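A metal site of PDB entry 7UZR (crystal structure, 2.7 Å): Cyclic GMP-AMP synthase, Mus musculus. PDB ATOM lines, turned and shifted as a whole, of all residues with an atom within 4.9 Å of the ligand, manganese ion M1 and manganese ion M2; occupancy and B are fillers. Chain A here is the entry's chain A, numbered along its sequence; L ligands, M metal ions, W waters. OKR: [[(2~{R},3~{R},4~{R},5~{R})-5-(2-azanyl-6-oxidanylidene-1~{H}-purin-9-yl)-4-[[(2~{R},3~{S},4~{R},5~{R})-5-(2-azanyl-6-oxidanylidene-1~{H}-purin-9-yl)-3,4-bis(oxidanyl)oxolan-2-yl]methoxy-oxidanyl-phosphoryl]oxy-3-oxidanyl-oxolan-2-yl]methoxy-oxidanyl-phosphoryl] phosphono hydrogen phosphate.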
ATOM      1  N   GLY A  55      -1.422  26.645  31.239  1.00  0.00           N
ATOM      2  CA  GLY A  55      -1.958  25.767  30.234  1.00  0.00           C
ATOM      3  C   GLY A  55      -1.674  24.309  30.520  1.00  0.00           C
ATOM      4  O   GLY A  55      -1.066  23.955  31.541  1.00  0.00           O
ATOM      5  N   SER A  56      -2.074  23.472  29.557  1.00  0.00           N
ATOM      6  CA  SER A  56      -2.120  22.030  29.692  1.00  0.00           C
ATOM      7  C   SER A  56      -0.785  21.421  30.012  1.00  0.00           C
ATOM      8  O   SER A  56      -0.731  20.473  30.791  1.00  0.00           O
ATOM      9  CB  SER A  56      -2.684  21.402  28.405  1.00  0.00           C
ATOM     10  OG  SER A  56      -1.928  21.795  27.235  1.00  0.00           O
ATOM     11  N   GLU A  59       0.113  21.998  33.515  1.00  0.00           N
ATOM     12  CA  GLU A  59      -0.924  21.330  34.324  1.00  0.00           C
ATOM     13  C   GLU A  59      -0.853  19.785  34.235  1.00  0.00           C
ATOM     14  O   GLU A  59      -1.593  19.067  34.916  1.00  0.00           O
ATOM     15  CB  GLU A  59      -2.310  21.774  33.881  1.00  0.00           C
ATOM     16  CG  GLU A  59      -2.671  23.221  34.167  1.00  0.00           C
ATOM     17  CD  GLU A  59      -3.915  23.746  33.416  1.00  0.00           C
ATOM     18  OE1 GLU A  59      -4.442  23.036  32.497  1.00  0.00           O
ATOM     19  OE2 GLU A  59      -4.347  24.889  33.748  1.00  0.00           O
ATOM     20  N   LYS A  62      -1.530  17.874  28.900  1.00  0.00           N
ATOM     21  CA  LYS A  62      -1.219  17.930  27.482  1.00  0.00           C
ATOM     22  C   LYS A  62      -1.175  16.525  26.939  1.00  0.00           C
ATOM     23  O   LYS A  62      -0.503  15.664  27.501  1.00  0.00           O
ATOM     24  CB  LYS A  62       0.139  18.594  27.264  1.00  0.00           C
ATOM     25  CG  LYS A  62       0.532  18.812  25.825  1.00  0.00           C
ATOM     26  CD  LYS A  62      -0.276  19.932  25.221  1.00  0.00           C
ATOM     27  CE  LYS A  62      -0.006  20.060  23.729  1.00  0.00           C
ATOM     28  NZ  LYS A  62      -0.437  18.859  22.971  1.00  0.00           N
ATOM     29  N   GLU A  68       2.432  22.329  22.017  1.00  0.00           N
ATOM     30  CA  GLU A  68       1.820  23.612  22.291  1.00  0.00           C
ATOM     31  C   GLU A  68       2.088  23.934  23.773  1.00  0.00           C
ATOM     32  O   GLU A  68       1.886  23.112  24.631  1.00  0.00           O
ATOM     33  CB  GLU A  68       0.317  23.662  21.912  1.00  0.00           C
ATOM     34  CG  GLU A  68      -0.271  25.078  21.685  1.00  0.00           C
ATOM     35  CD  GLU A  68      -0.986  25.687  22.884  1.00  0.00           C
ATOM     36  OE1 GLU A  68      -0.948  25.064  23.972  1.00  0.00           O
ATOM     37  OE2 GLU A  68      -1.591  26.790  22.758  1.00  0.00           O
ATOM     38  N   ASP A  70       1.867  27.317  26.650  1.00  0.00           N
ATOM     39  CA  ASP A  70       1.282  28.615  26.895  1.00  0.00           C
ATOM     40  C   ASP A  70       2.115  29.320  27.997  1.00  0.00           C
ATOM     41  O   ASP A  70       2.464  28.702  28.974  1.00  0.00           O
ATOM     42  CB  ASP A  70      -0.193  28.433  27.250  1.00  0.00           C
ATOM     43  CG  ASP A  70      -0.964  27.586  26.199  1.00  0.00           C
ATOM     44  OD1 ASP A  70      -1.230  28.062  25.079  1.00  0.00           O
ATOM     45  OD2 ASP A  70      -1.312  26.441  26.502  1.00  0.00           O
ATOM     46  N   LYS A 145      -4.020  36.429  14.538  1.00  0.00           N
ATOM     47  CA  LYS A 145      -5.383  35.968  14.431  1.00  0.00           C
ATOM     48  C   LYS A 145      -6.218  36.966  15.209  1.00  0.00           C
ATOM     49  O   LYS A 145      -5.912  37.257  16.367  1.00  0.00           O
ATOM     50  CB  LYS A 145      -5.534  34.605  15.084  1.00  0.00           C
ATOM     51  CG  LYS A 145      -4.749  33.550  14.345  1.00  0.00           C
ATOM     52  CD  LYS A 145      -5.248  32.173  14.706  1.00  0.00           C
ATOM     53  CE  LYS A 145      -4.289  31.085  14.251  1.00  0.00           C
ATOM     54  NZ  LYS A 145      -3.604  31.392  12.966  1.00  0.00           N
ATOM     55  N   GLY A 147      -9.264  38.284  17.573  1.00  0.00           N
ATOM     56  CA  GLY A 147      -9.817  37.678  18.769  1.00  0.00           C
ATOM     57  C   GLY A 147      -8.826  36.801  19.500  1.00  0.00           C
ATOM     58  O   GLY A 147      -9.242  35.881  20.199  1.00  0.00           O
ATOM     59  N   ASP A 164       2.228  30.155  22.646  1.00  0.00           N
ATOM     60  CA  ASP A 164       1.473  31.368  22.809  1.00  0.00           C
ATOM     61  C   ASP A 164       2.149  32.201  23.889  1.00  0.00           C
ATOM     62  O   ASP A 164       2.182  31.793  25.050  1.00  0.00           O
ATOM     63  CB  ASP A 164       0.044  31.031  23.204  1.00  0.00           C
ATOM     64  CG  ASP A 164      -0.686  30.254  22.141  1.00  0.00           C
ATOM     65  OD1 ASP A 164      -0.377  30.476  20.941  1.00  0.00           O
ATOM     66  OD2 ASP A 164      -1.573  29.433  22.521  1.00  0.00           O
ATOM     67  N   ARG A 221     -10.010  41.224  28.809  1.00  0.00           N
ATOM     68  CA  ARG A 221     -10.770  40.034  29.302  1.00  0.00           C
ATOM     69  C   ARG A 221     -10.015  39.442  30.508  1.00  0.00           C
ATOM     70  O   ARG A 221      -8.775  39.397  30.450  1.00  0.00           O
ATOM     71  CB  ARG A 221     -10.929  38.975  28.202  1.00  0.00           C
ATOM     72  CG  ARG A 221     -11.838  37.804  28.560  1.00  0.00           C
ATOM     73  CD  ARG A 221     -11.802  36.661  27.557  1.00  0.00           C
ATOM     74  NE  ARG A 221     -10.479  36.048  27.460  1.00  0.00           N
ATOM     75  CZ  ARG A 221      -9.948  35.153  28.312  1.00  0.00           C
ATOM     76  NH1 ARG A 221     -10.655  34.745  29.359  1.00  0.00           N
ATOM     77  NH2 ARG A 221      -8.728  34.680  28.117  1.00  0.00           N
ATOM     78  N   SER A 225      -5.856  31.732  34.665  1.00  0.00           N
ATOM     79  CA  SER A 225      -4.963  30.630  34.305  1.00  0.00           C
ATOM     80  C   SER A 225      -4.117  30.152  35.464  1.00  0.00           C
ATOM     81  O   SER A 225      -3.813  28.969  35.552  1.00  0.00           O
ATOM     82  CB  SER A 225      -4.040  31.059  33.211  1.00  0.00           C
ATOM     83  OG  SER A 225      -4.665  30.885  31.979  1.00  0.00           O
ATOM     84  N   LYS A 259     -10.586  15.885  26.192  1.00  0.00           N
ATOM     85  CA  LYS A 259      -9.779  16.783  25.353  1.00  0.00           C
ATOM     86  C   LYS A 259      -9.523  16.146  23.987  1.00  0.00           C
ATOM     87  O   LYS A 259      -9.581  16.839  22.945  1.00  0.00           O
ATOM     88  CB  LYS A 259      -8.424  17.078  25.990  1.00  0.00           C
ATOM     89  CG  LYS A 259      -8.459  18.095  27.097  1.00  0.00           C
ATOM     90  CD  LYS A 259      -7.141  18.094  27.867  1.00  0.00           C
ATOM     91  CE  LYS A 259      -6.001  18.831  27.122  1.00  0.00           C
ATOM     92  NZ  LYS A 259      -6.115  20.335  27.123  1.00  0.00           N
ATOM     93  N   GLU A 263     -10.485  17.240  20.204  1.00  0.00           N
ATOM     94  CA  GLU A 263      -9.400  17.422  19.213  1.00  0.00           C
ATOM     95  C   GLU A 263      -9.570  16.588  17.935  1.00  0.00           C
ATOM     96  O   GLU A 263      -9.467  17.116  16.841  1.00  0.00           O
ATOM     97  CB  GLU A 263      -8.015  17.086  19.806  1.00  0.00           C
ATOM     98  CG  GLU A 263      -7.407  18.203  20.644  1.00  0.00           C
ATOM     99  CD  GLU A 263      -6.011  17.875  21.160  1.00  0.00           C
ATOM    100  OE1 GLU A 263      -5.343  17.065  20.491  1.00  0.00           O
ATOM    101  OE2 GLU A 263      -5.615  18.438  22.224  1.00  0.00           O
ATOM    102  N   LYS A 266     -12.507  17.900  16.036  1.00  0.00           N
ATOM    103  CA  LYS A 266     -12.158  19.190  15.489  1.00  0.00           C
ATOM    104  C   LYS A 266     -11.247  19.084  14.257  1.00  0.00           C
ATOM    105  O   LYS A 266     -11.406  19.878  13.322  1.00  0.00           O
ATOM    106  CB  LYS A 266     -11.473  20.050  16.540  1.00  0.00           C
ATOM    107  CG  LYS A 266     -12.329  20.545  17.690  1.00  0.00           C
ATOM    108  CD  LYS A 266     -12.545  22.053  17.710  1.00  0.00           C
ATOM    109  CE  LYS A 266     -11.267  22.854  17.919  1.00  0.00           C
ATOM    110  NZ  LYS A 266     -11.460  24.088  17.087  1.00  0.00           N
ATOM    111  N   PHE A 275     -15.801  25.573  18.852  1.00  0.00           N
ATOM    112  CA  PHE A 275     -15.470  24.876  20.088  1.00  0.00           C
ATOM    113  C   PHE A 275     -13.973  24.783  20.381  1.00  0.00           C
ATOM    114  O   PHE A 275     -13.176  24.751  19.474  1.00  0.00           O
ATOM    115  CB  PHE A 275     -16.062  23.498  20.082  1.00  0.00           C
ATOM    116  CG  PHE A 275     -17.540  23.481  19.926  1.00  0.00           C
ATOM    117  CD1 PHE A 275     -18.356  23.687  21.018  1.00  0.00           C
ATOM    118  CD2 PHE A 275     -18.106  23.200  18.698  1.00  0.00           C
ATOM    119  CE1 PHE A 275     -19.726  23.666  20.878  1.00  0.00           C
ATOM    120  CE2 PHE A 275     -19.470  23.150  18.560  1.00  0.00           C
ATOM    121  CZ  PHE A 275     -20.285  23.393  19.650  1.00  0.00           C
ATOM    122  N   CYS A 276     -13.625  24.757  21.673  1.00  0.00           N
ATOM    123  CA  CYS A 276     -12.240  24.744  22.134  1.00  0.00           C
ATOM    124  C   CYS A 276     -12.131  23.901  23.395  1.00  0.00           C
ATOM    125  O   CYS A 276     -13.118  23.548  24.002  1.00  0.00           O
ATOM    126  CB  CYS A 276     -11.740  26.169  22.371  1.00  0.00           C
ATOM    127  SG  CYS A 276     -12.550  27.067  23.721  1.00  0.00           S
ATOM    128  N   SER A 277     -10.887  23.625  23.817  1.00  0.00           N
ATOM    129  CA  SER A 277     -10.645  22.797  24.984  1.00  0.00           C
ATOM    130  C   SER A 277     -11.078  23.504  26.252  1.00  0.00           C
ATOM    131  O   SER A 277     -11.315  22.843  27.284  1.00  0.00           O
ATOM    132  CB  SER A 277      -9.183  22.390  25.069  1.00  0.00           C
ATOM    133  OG  SER A 277      -8.383  23.532  24.932  1.00  0.00           O
ATOM    134  N   TYR A 278     -11.159  24.828  26.220  1.00  0.00           N
ATOM    135  CA  TYR A 278     -11.544  25.593  27.427  1.00  0.00           C
ATOM    136  C   TYR A 278     -12.979  25.196  27.809  1.00  0.00           C
ATOM    137  O   TYR A 278     -13.308  25.201  29.007  1.00  0.00           O
ATOM    138  CB  TYR A 278     -11.429  27.105  27.255  1.00  0.00           C
ATOM    139  CG  TYR A 278     -11.496  27.786  28.601  1.00  0.00           C
ATOM    140  CD1 TYR A 278     -10.467  27.591  29.503  1.00  0.00           C
ATOM    141  CD2 TYR A 278     -12.602  28.514  29.008  1.00  0.00           C
ATOM    142  CE1 TYR A 278     -10.495  28.169  30.755  1.00  0.00           C
ATOM    143  CE2 TYR A 278     -12.656  29.100  30.270  1.00  0.00           C
ATOM    144  CZ  TYR A 278     -11.593  28.914  31.146  1.00  0.00           C
ATOM    145  OH  TYR A 278     -11.582  29.461  32.389  1.00  0.00           O
ATOM    146  N   LYS A 281     -12.663  21.984  29.740  1.00  0.00           N
ATOM    147  CA  LYS A 281     -12.008  22.256  31.035  1.00  0.00           C
ATOM    148  C   LYS A 281     -13.001  22.883  32.022  1.00  0.00           C
ATOM    149  O   LYS A 281     -13.092  22.467  33.178  1.00  0.00           O
ATOM    150  CB  LYS A 281     -10.855  23.214  30.839  1.00  0.00           C
ATOM    151  CG  LYS A 281      -9.943  23.382  32.036  1.00  0.00           C
ATOM    152  CD  LYS A 281      -9.001  24.560  31.832  1.00  0.00           C
ATOM    153  CE  LYS A 281      -7.604  24.256  32.350  1.00  0.00           C
ATOM    154  NZ  LYS A 281      -6.836  25.485  32.729  1.00  0.00           N
ATOM    155  N   HIS A 324     -19.034  30.196  32.693  1.00  0.00           N
ATOM    156  CA  HIS A 324     -17.637  30.355  33.104  1.00  0.00           C
ATOM    157  C   HIS A 324     -17.567  30.010  34.591  1.00  0.00           C
ATOM    158  O   HIS A 324     -18.414  30.415  35.374  1.00  0.00           O
ATOM    159  CB  HIS A 324     -17.174  31.787  32.867  1.00  0.00           C
ATOM    160  CG  HIS A 324     -15.692  31.938  32.806  1.00  0.00           C
ATOM    161  ND1 HIS A 324     -14.902  31.862  33.930  1.00  0.00           N
ATOM    162  CD2 HIS A 324     -14.854  32.148  31.766  1.00  0.00           C
ATOM    163  CE1 HIS A 324     -13.640  32.028  33.576  1.00  0.00           C
ATOM    164  NE2 HIS A 324     -13.585  32.203  32.274  1.00  0.00           N
HETATM  165  N1  OKR L   1      -4.346  24.934  21.934  1.00  0.00           N
HETATM  166  C1  OKR L   1      -5.593  25.014  21.428  1.00  0.00           C
HETATM  167  N2  OKR L   1      -5.876  25.971  20.546  1.00  0.00           N
HETATM  168  C2  OKR L   1      -7.161  25.916  20.134  1.00  0.00           C
HETATM  169  C3  OKR L   1      -8.154  25.036  20.511  1.00  0.00           C
HETATM  170  N3  OKR L   1      -9.347  25.321  19.856  1.00  0.00           N
HETATM  171  C4  OKR L   1      -9.065  26.361  19.112  1.00  0.00           C
HETATM  172  N4  OKR L   1      -7.749  26.773  19.244  1.00  0.00           N
HETATM  173  C5  OKR L   1      -7.061  27.883  18.576  1.00  0.00           C
HETATM  174  O1  OKR L   1      -7.298  29.067  19.306  1.00  0.00           O
HETATM  175  C6  OKR L   1      -7.137  30.206  18.427  1.00  0.00           C
HETATM  176  C7  OKR L   1      -8.287  31.168  18.630  1.00  0.00           C
HETATM  177  O2  OKR L   1      -8.600  31.289  20.048  1.00  0.00           O
HETATM  178  P1  OKR L   1      -9.902  30.598  20.687  1.00  0.00           P
HETATM  179  O3  OKR L   1     -10.559  31.614  21.573  1.00  0.00           O
HETATM  180  O4  OKR L   1     -10.777  29.955  19.636  1.00  0.00           O
HETATM  181  O5  OKR L   1      -9.246  29.407  21.535  1.00  0.00           O
HETATM  182  C8  OKR L   1      -9.022  29.663  22.926  1.00  0.00           C
HETATM  183  C9  OKR L   1      -7.778  28.924  23.365  1.00  0.00           C
HETATM  184  O6  OKR L   1      -6.759  28.929  22.374  1.00  0.00           O
HETATM  185  C10 OKR L   1      -8.339  27.517  23.616  1.00  0.00           C
HETATM  186  C11 OKR L   1      -7.501  26.622  24.493  1.00  0.00           C
HETATM  187  O7  OKR L   1      -6.105  26.861  24.224  1.00  0.00           O
HETATM  188  P2  OKR L   1      -5.022  26.811  25.403  1.00  0.00           P
HETATM  189  O8  OKR L   1      -5.220  28.030  26.244  1.00  0.00           O
HETATM  190  O9  OKR L   1      -3.668  26.519  24.849  1.00  0.00           O
HETATM  191  O10 OKR L   1      -5.506  25.502  26.203  1.00  0.00           O
HETATM  192  P3  OKR L   1      -4.922  24.540  27.344  1.00  0.00           P
HETATM  193  O11 OKR L   1      -5.836  24.644  28.531  1.00  0.00           O
HETATM  194  O12 OKR L   1      -3.453  24.769  27.529  1.00  0.00           O
HETATM  195  O13 OKR L   1      -5.109  23.135  26.622  1.00  0.00           O
HETATM  196  P4  OKR L   1      -4.635  22.685  25.147  1.00  0.00           P
HETATM  197  O14 OKR L   1      -3.837  23.843  24.622  1.00  0.00           O
HETATM  198  O15 OKR L   1      -5.916  22.445  24.380  1.00  0.00           O
HETATM  199  O16 OKR L   1      -3.791  21.431  25.287  1.00  0.00           O
HETATM  200  O17 OKR L   1      -9.622  27.777  24.240  1.00  0.00           O
HETATM  201  C12 OKR L   1     -10.125  29.012  23.774  1.00  0.00           C
HETATM  202  N5  OKR L   1     -10.553  29.824  24.903  1.00  0.00           N
HETATM  203  C13 OKR L   1     -11.744  30.500  24.987  1.00  0.00           C
HETATM  204  N6  OKR L   1     -11.900  31.169  26.105  1.00  0.00           N
HETATM  205  C14 OKR L   1     -10.717  30.922  26.799  1.00  0.00           C
HETATM  206  C15 OKR L   1     -10.311  31.391  28.081  1.00  0.00           C
HETATM  207  O18 OKR L   1     -10.938  32.121  28.862  1.00  0.00           O
HETATM  208  N7  OKR L   1      -9.046  30.913  28.419  1.00  0.00           N
HETATM  209  C16 OKR L   1      -8.283  30.081  27.633  1.00  0.00           C
HETATM  210  N8  OKR L   1      -7.091  29.714  28.128  1.00  0.00           N
HETATM  211  N9  OKR L   1      -8.655  29.634  26.432  1.00  0.00           N
HETATM  212  C17 OKR L   1      -9.877  30.103  26.079  1.00  0.00           C
HETATM  213  C18 OKR L   1      -6.991  29.632  17.001  1.00  0.00           C
HETATM  214  O19 OKR L   1      -5.633  29.590  16.567  1.00  0.00           O
HETATM  215  C19 OKR L   1      -7.530  28.196  17.158  1.00  0.00           C
HETATM  216  O20 OKR L   1      -6.983  27.317  16.205  1.00  0.00           O
HETATM  217  C20 OKR L   1      -7.841  24.013  21.449  1.00  0.00           C
HETATM  218  O21 OKR L   1      -8.590  23.136  21.896  1.00  0.00           O
HETATM  219  N10 OKR L   1      -6.506  24.082  21.862  1.00  0.00           N
HETATM  220 MN    MN M   1      -2.678  28.278  23.546  1.00  0.00          MN
HETATM  221 MN    MN M   2      -2.167  24.870  25.471  1.00  0.00          MN
HETATM  222  O   HOH W   1      -5.635  22.347  30.158  1.00  0.00           O
HETATM  223  O   HOH W   2      -3.235  18.796  24.404  1.00  0.00           O
HETATM  224  O   HOH W   3      -0.398  23.858  26.482  1.00  0.00           O
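NH1 of Arg 221 is in hydrogen-bond range of O18 of the ligand (2.7 Å).
An oxygen (O12) of the ligand lies close to the backbone NH of Ser 56 (2.8 Å).
The side-chain hydroxyl (OG) of Ser 277 is in hydrogen-bond range of an oxygen (O15) of the ligand (2.8 Å).
O21 of the ligand lies within hydrogen-bond range of N of Ser 277 (3.0 Å).
An oxygen (O17) of the ligand sits at hydrogen-bond distance from the side-chain sulfur (SG) of Cys 276, 3.1 Å away.
The side-chain amino group of Lys 259 is in salt-bridge range of an oxygen (O16) of the ligand, 3.2 Å away.
OG of Ser 56 is in hydrogen-bond range of O16 of the ligand (2.7 Å).
The side-chain amino group (NZ) of Lys 266 is in hydrogen-bond range of the backbone carbonyl oxygen (O) of Phe 275 (3.0 Å).
The backbone NH of Tyr 278 sits close to the side-chain sulfur of Cys 276 (3.6 Å).
O of Ser 56 sits at hydrogen-bond distance from N of Lys 62, 3.3 Å away.
OH of Tyr 278 is in hydrogen-bond range of NE2 of His 324, 3.4 Å away.
Residues that only touch the ligand: Lys 145, Gly 55, Tyr 278, Lys 266, Lys 62 and Phe 275.
Within 4 Å of the ligand: Gly 55, Ser 56, Lys 62, Glu 68, Asp 70, Lys 145, Arg 221, Lys 259, Lys 266, Phe 275, Cys 276, Ser 277 and Tyr 278.
Within 4 Å of manganese ion M1: Glu 68, Asp 70 and Asp 164.
Residues that only touch manganese ion M2: Ser 56.
Three residues have an atom within 4 Å of manganese ion M2: Ser 56, Glu 68 and Asp 70.
The nearest printed residue that does not touch manganese ion M2 is Gly 55 (4.9 Å).
Manganese ion M1 is bound by the side-chain carboxylate (OD2) of Asp 164 (1.9 Å), the side-chain carboxylate (OE2) of Glu 68 (2.0 Å), the side-chain carboxylate (OD1) of Asp 70 (2.1 Å) and an oxygen (O9) of the ligand (2.4 Å).
OE1 of Glu 68 binds manganese ion M2 (1.9 Å).
The side-chain carboxylate (OD2) of Asp 70 is bound to manganese ion M2 (2.1 Å).
Manganese ion M2 is bound by O14 of the ligand.
Water W3 binds manganese ion M2.
O9 of the ligand binds manganese ion M2 (2.3 Å).
O12 of the ligand binds manganese ion M2, at 2.4 Å.
Manganese ion M2 has six donor atoms within binding distance.
Water W3 bridges the side-chain hydroxyl of Ser 56 (2.7 Å) and the backbone carbonyl oxygen of Glu 68 (3.0 Å).
Water W1 bridges the side-chain carboxylate (OE1) of Glu 59 (2.7 Å) and an oxygen (O11) of the ligand (2.8 Å).
Water W2 lies within hydrogen-bond range of O16 of the ligand, NZ of Lys 62 and OE2 of Glu 263.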
